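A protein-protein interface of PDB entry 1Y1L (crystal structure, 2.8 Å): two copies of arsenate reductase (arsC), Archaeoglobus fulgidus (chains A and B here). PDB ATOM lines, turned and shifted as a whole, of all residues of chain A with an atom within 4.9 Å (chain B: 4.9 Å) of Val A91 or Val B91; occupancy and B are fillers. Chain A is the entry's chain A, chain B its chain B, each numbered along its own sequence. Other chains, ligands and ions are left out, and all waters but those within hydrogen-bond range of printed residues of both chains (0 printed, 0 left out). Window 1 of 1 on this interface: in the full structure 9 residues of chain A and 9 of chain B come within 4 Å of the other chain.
The backbone NH (N) of Thr A92 is in hydrogen-bond range of the backbone carbonyl oxygen (O) of Ile A73 (3.2 Å).
O of Pro B90 is in hydrogen-bond range of N of Ile B73 (2.9 Å).
N of Ile A73 sits at hydrogen-bond distance from O of Pro A90, at 2.9 Å.
N of Thr B75 sits at hydrogen-bond distance from O of Thr B92.
OG1 of Thr A87 sits close to N of Lys A89, at 3.2 Å.
The side-chain hydroxyl (OG1) of Thr B87 sits close to the backbone NH (N) of Lys B89, 3.2 Å away.
Among the printed residues, pairs that only touch across the chains: Lys A89 with Val B91 (3.7 Å), Lys A89 with Thr B92 (3.4 Å), Pro A90 with Val B91 (3.6 Å), Pro A90 with Thr B92 (3.0 Å), Val A91 with Lys B89 (3.6 Å), Val A91 with Pro B90 (3.6 Å), Val A91 with Val B91 (3.6 Å), Thr A92 with Lys B89 (3.5 Å) and Thr A92 with Pro B90 (3.0 Å).
Of chain B, only Lys B89, Pro B90 and Val B91 come within 4 Å of Val A91.
Of chain A, only Lys A89 (3.7 Å), Pro A90 (3.6 Å) and Val A91 (3.6 Å) come within 4 Å of Val B91.
Of the printed residues of chain A, Lys B89 touches Val A91 and Thr A92.
Of the printed residues of chain B, Thr A92 touches Lys B89 (3.5 Å) and Pro B90 (3.0 Å).
The nearest printed residue of chain B that does not touch Val A91 is Thr B92 (5.3 Å).
The nearest printed residue of chain A that does not touch Pro B90 is Leu A72 (4.7 Å).
Of the 9 printed residues of chain A, 4 touch a printed residue of chain B.
Hydrophobic or aromatic side chains of chain A within 4 Å of the printed part of chain B: Pro A90.
Printed residues of chain B that touch a printed residue of chain A: Lys B89, Pro B90, Val B91 and Thr B92.
Hydrophobic or aromatic side chains of chain B within 4 Å of the printed part of chain A: Pro B90.
Among the printed residues, no Asp or Glu carboxylate lies within 4 Å of a Lys or Arg side-chain nitrogen of the other chain.
Lys A89 touches Val B91, and with the chains exchanged Val A91 touches Lys B89.
Lys A89 touches Thr B92, and with the chains exchanged Thr A92 touches Lys B89.
Pro A90 touches Val B91, and with the chains exchanged Val A91 touches Pro B90.
Pro A90 touches Thr B92, and with the chains exchanged Thr A92 touches Pro B90.
9 positions are printed for both chains.
Of the 9 pairs that touch across the chains among the printed residues, 9 have their exchanged pair printed and touching as well.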
ATOM      1  N   LEU A  72     -16.711  18.989  24.228  1.00  0.00           N
ATOM      2  CA  LEU A  72     -17.768  17.988  24.052  1.00  0.00           C
ATOM      3  C   LEU A  72     -17.615  17.461  22.654  1.00  0.00           C
ATOM      4  O   LEU A  72     -17.856  18.184  21.703  1.00  0.00           O
ATOM      5  CB  LEU A  72     -19.167  18.595  24.227  1.00  0.00           C
ATOM      6  CG  LEU A  72     -20.438  17.749  24.066  1.00  0.00           C
ATOM      7  CD1 LEU A  72     -21.101  18.044  22.753  1.00  0.00           C
ATOM      8  CD2 LEU A  72     -20.156  16.278  24.216  1.00  0.00           C
ATOM      9  N   ILE A  73     -17.108  16.246  22.525  1.00  0.00           N
ATOM     10  CA  ILE A  73     -16.956  15.666  21.206  1.00  0.00           C
ATOM     11  C   ILE A  73     -18.066  14.647  20.990  1.00  0.00           C
ATOM     12  O   ILE A  73     -18.122  13.627  21.663  1.00  0.00           O
ATOM     13  CB  ILE A  73     -15.520  15.094  20.977  1.00  0.00           C
ATOM     14  CG1 ILE A  73     -15.435  14.301  19.667  1.00  0.00           C
ATOM     15  CG2 ILE A  73     -15.060  14.294  22.169  1.00  0.00           C
ATOM     16  CD1 ILE A  73     -15.797  12.828  19.783  1.00  0.00           C
ATOM     17  N   THR A  75     -19.905  11.962  18.843  1.00  0.00           N
ATOM     18  CA  THR A  75     -19.524  10.978  17.825  1.00  0.00           C
ATOM     19  C   THR A  75     -20.742  10.412  17.086  1.00  0.00           C
ATOM     20  O   THR A  75     -21.652   9.842  17.699  1.00  0.00           O
ATOM     21  CB  THR A  75     -18.704   9.813  18.446  1.00  0.00           C
ATOM     22  OG1 THR A  75     -17.392  10.271  18.782  1.00  0.00           O
ATOM     23  CG2 THR A  75     -18.575   8.657  17.473  1.00  0.00           C
ATOM     24  N   THR A  87      -9.398  10.242  24.258  1.00  0.00           N
ATOM     25  CA  THR A  87      -9.625  11.347  25.162  1.00  0.00           C
ATOM     26  C   THR A  87     -10.478  10.986  26.379  1.00  0.00           C
ATOM     27  O   THR A  87     -11.528  10.359  26.229  1.00  0.00           O
ATOM     28  CB  THR A  87     -10.264  12.525  24.391  1.00  0.00           C
ATOM     29  OG1 THR A  87     -10.217  13.712  25.192  1.00  0.00           O
ATOM     30  CG2 THR A  87     -11.708  12.226  24.019  1.00  0.00           C
ATOM     31  N   LYS A  89     -11.868  13.007  27.852  1.00  0.00           N
ATOM     32  CA  LYS A  89     -12.830  14.122  27.723  1.00  0.00           C
ATOM     33  C   LYS A  89     -14.274  13.628  27.545  1.00  0.00           C
ATOM     34  O   LYS A  89     -14.522  12.425  27.396  1.00  0.00           O
ATOM     35  CB  LYS A  89     -12.492  14.969  26.494  1.00  0.00           C
ATOM     36  CG  LYS A  89     -11.525  16.108  26.740  1.00  0.00           C
ATOM     37  CD  LYS A  89     -12.184  17.265  27.492  1.00  0.00           C
ATOM     38  CE  LYS A  89     -11.274  18.492  27.557  1.00  0.00           C
ATOM     39  NZ  LYS A  89     -11.996  19.688  28.073  1.00  0.00           N
ATOM     40  N   PRO A  90     -15.246  14.550  27.514  1.00  0.00           N
ATOM     41  CA  PRO A  90     -16.644  14.141  27.344  1.00  0.00           C
ATOM     42  C   PRO A  90     -17.018  13.906  25.889  1.00  0.00           C
ATOM     43  O   PRO A  90     -16.728  14.739  25.030  1.00  0.00           O
ATOM     44  CB  PRO A  90     -17.415  15.320  27.929  1.00  0.00           C
ATOM     45  CG  PRO A  90     -16.556  16.470  27.580  1.00  0.00           C
ATOM     46  CD  PRO A  90     -15.166  15.968  27.889  1.00  0.00           C
ATOM     47  N   VAL A  91     -17.654  12.768  25.620  1.00  0.00           N
ATOM     48  CA  VAL A  91     -18.077  12.411  24.270  1.00  0.00           C
ATOM     49  C   VAL A  91     -19.378  11.597  24.252  1.00  0.00           C
ATOM     50  O   VAL A  91     -19.560  10.687  25.063  1.00  0.00           O
ATOM     51  CB  VAL A  91     -16.941  11.678  23.462  1.00  0.00           C
ATOM     52  CG1 VAL A  91     -15.722  11.390  24.324  1.00  0.00           C
ATOM     53  CG2 VAL A  91     -17.464  10.409  22.831  1.00  0.00           C
ATOM     54  N   THR A  92     -20.290  11.962  23.352  1.00  0.00           N
ATOM     55  CA  THR A  92     -21.572  11.270  23.207  1.00  0.00           C
ATOM     56  C   THR A  92     -21.574  10.426  21.926  1.00  0.00           C
ATOM     57  O   THR A  92     -20.599  10.425  21.161  1.00  0.00           O
ATOM     58  CB  THR A  92     -22.753  12.253  23.120  1.00  0.00           C
ATOM     59  OG1 THR A  92     -22.543  13.359  24.003  1.00  0.00           O
ATOM     60  CG2 THR A  92     -24.037  11.566  23.528  1.00  0.00           C
ATOM     61  N   ARG A  93     -22.675   9.718  21.685  1.00  0.00           N
ATOM     62  CA  ARG A  93     -22.800   8.874  20.502  1.00  0.00           C
ATOM     63  C   ARG A  93     -24.167   9.003  19.850  1.00  0.00           C
ATOM     64  O   ARG A  93     -25.192   8.803  20.499  1.00  0.00           O
ATOM     65  CB  ARG A  93     -22.553   7.421  20.884  1.00  0.00           C
ATOM     66  CG  ARG A  93     -21.166   7.179  21.450  1.00  0.00           C
ATOM     67  CD  ARG A  93     -21.002   5.750  21.916  1.00  0.00           C
ATOM     68  NE  ARG A  93     -19.645   5.472  22.384  1.00  0.00           N
ATOM     69  CZ  ARG A  93     -19.354   4.655  23.396  1.00  0.00           C
ATOM     70  NH1 ARG A  93     -18.084   4.467  23.744  1.00  0.00           N
ATOM     71  NH2 ARG A  93     -20.322   4.033  24.071  1.00  0.00           N
ATOM     72  N   LEU B  72     -25.298  14.303  31.419  1.00  0.00           N
ATOM     73  CA  LEU B  72     -23.835  14.332  31.414  1.00  0.00           C
ATOM     74  C   LEU B  72     -23.414  13.493  32.593  1.00  0.00           C
ATOM     75  O   LEU B  72     -23.648  13.873  33.733  1.00  0.00           O
ATOM     76  CB  LEU B  72     -23.304  15.770  31.582  1.00  0.00           C
ATOM     77  CG  LEU B  72     -21.804  16.096  31.650  1.00  0.00           C
ATOM     78  CD1 LEU B  72     -21.382  16.359  33.067  1.00  0.00           C
ATOM     79  CD2 LEU B  72     -20.972  15.003  31.031  1.00  0.00           C
ATOM     80  N   ILE B  73     -22.890  12.309  32.331  1.00  0.00           N
ATOM     81  CA  ILE B  73     -22.454  11.462  33.429  1.00  0.00           C
ATOM     82  C   ILE B  73     -20.929  11.503  33.503  1.00  0.00           C
ATOM     83  O   ILE B  73     -20.235  11.065  32.595  1.00  0.00           O
ATOM     84  CB  ILE B  73     -23.057  10.011  33.338  1.00  0.00           C
ATOM     85  CG1 ILE B  73     -22.424   9.082  34.365  1.00  0.00           C
ATOM     86  CG2 ILE B  73     -22.935   9.455  31.941  1.00  0.00           C
ATOM     87  CD1 ILE B  73     -21.143   8.429  33.898  1.00  0.00           C
ATOM     88  N   THR B  75     -17.547  10.417  35.049  1.00  0.00           N
ATOM     89  CA  THR B  75     -17.022   9.222  35.697  1.00  0.00           C
ATOM     90  C   THR B  75     -15.682   9.493  36.380  1.00  0.00           C
ATOM     91  O   THR B  75     -14.708   9.862  35.713  1.00  0.00           O
ATOM     92  CB  THR B  75     -16.840   8.066  34.665  1.00  0.00           C
ATOM     93  OG1 THR B  75     -18.122   7.566  34.266  1.00  0.00           O
ATOM     94  CG2 THR B  75     -16.028   6.925  35.260  1.00  0.00           C
ATOM     95  N   THR B  87     -24.359   3.377  28.219  1.00  0.00           N
ATOM     96  CA  THR B  87     -25.086   4.514  27.665  1.00  0.00           C
ATOM     97  C   THR B  87     -24.390   5.207  26.490  1.00  0.00           C
ATOM     98  O   THR B  87     -23.189   5.475  26.548  1.00  0.00           O
ATOM     99  CB  THR B  87     -25.427   5.543  28.767  1.00  0.00           C
ATOM    100  OG1 THR B  87     -26.407   6.469  28.276  1.00  0.00           O
ATOM    101  CG2 THR B  87     -24.169   6.293  29.230  1.00  0.00           C
ATOM    102  N   LYS B  89     -24.980   7.922  25.814  1.00  0.00           N
ATOM    103  CA  LYS B  89     -25.033   9.299  26.359  1.00  0.00           C
ATOM    104  C   LYS B  89     -23.638   9.930  26.572  1.00  0.00           C
ATOM    105  O   LYS B  89     -22.608   9.249  26.457  1.00  0.00           O
ATOM    106  CB  LYS B  89     -25.741   9.294  27.719  1.00  0.00           C
ATOM    107  CG  LYS B  89     -27.246   9.467  27.673  1.00  0.00           C
ATOM    108  CD  LYS B  89     -27.640  10.898  27.324  1.00  0.00           C
ATOM    109  CE  LYS B  89     -29.129  11.118  27.537  1.00  0.00           C
ATOM    110  NZ  LYS B  89     -29.505  12.547  27.367  1.00  0.00           N
ATOM    111  N   PRO B  90     -23.586  11.241  26.900  1.00  0.00           N
ATOM    112  CA  PRO B  90     -22.292  11.903  27.124  1.00  0.00           C
ATOM    113  C   PRO B  90     -21.702  11.598  28.510  1.00  0.00           C
ATOM    114  O   PRO B  90     -22.398  11.714  29.527  1.00  0.00           O
ATOM    115  CB  PRO B  90     -22.642  13.389  26.970  1.00  0.00           C
ATOM    116  CG  PRO B  90     -24.006  13.457  27.499  1.00  0.00           C
ATOM    117  CD  PRO B  90     -24.668  12.241  26.881  1.00  0.00           C
ATOM    118  N   VAL B  91     -20.429  11.195  28.538  1.00  0.00           N
ATOM    119  CA  VAL B  91     -19.741  10.872  29.782  1.00  0.00           C
ATOM    120  C   VAL B  91     -18.261  11.221  29.733  1.00  0.00           C
ATOM    121  O   VAL B  91     -17.583  10.910  28.748  1.00  0.00           O
ATOM    122  CB  VAL B  91     -19.923   9.364  30.190  1.00  0.00           C
ATOM    123  CG1 VAL B  91     -20.652   8.584  29.127  1.00  0.00           C
ATOM    124  CG2 VAL B  91     -18.590   8.707  30.495  1.00  0.00           C
ATOM    125  N   THR B  92     -17.771  11.877  30.793  1.00  0.00           N
ATOM    126  CA  THR B  92     -16.352  12.263  30.896  1.00  0.00           C
ATOM    127  C   THR B  92     -15.646  11.382  31.923  1.00  0.00           C
ATOM    128  O   THR B  92     -16.282  10.576  32.608  1.00  0.00           O
ATOM    129  CB  THR B  92     -16.158  13.712  31.351  1.00  0.00           C
ATOM    130  OG1 THR B  92     -17.177  14.547  30.794  1.00  0.00           O
ATOM    131  CG2 THR B  92     -14.817  14.218  30.875  1.00  0.00           C
ATOM    132  N   ARG B  93     -14.336  11.564  32.059  1.00  0.00           N
ATOM    133  CA  ARG B  93     -13.534  10.780  32.997  1.00  0.00           C
ATOM    134  C   ARG B  93     -12.572  11.650  33.792  1.00  0.00           C
ATOM    135  O   ARG B  93     -11.759  12.380  33.217  1.00  0.00           O
ATOM    136  CB  ARG B  93     -12.734   9.731  32.230  1.00  0.00           C
ATOM    137  CG  ARG B  93     -13.594   8.749  31.461  1.00  0.00           C
ATOM    138  CD  ARG B  93     -12.751   7.822  30.620  1.00  0.00           C
ATOM    139  NE  ARG B  93     -13.563   6.822  29.934  1.00  0.00           N
ATOM    140  CZ  ARG B  93     -13.310   6.354  28.713  1.00  0.00           C
ATOM    141  NH1 ARG B  93     -14.114   5.438  28.183  1.00  0.00           N
ATOM    142  NH2 ARG B  93     -12.266   6.802  28.019  1.00  0.00           N
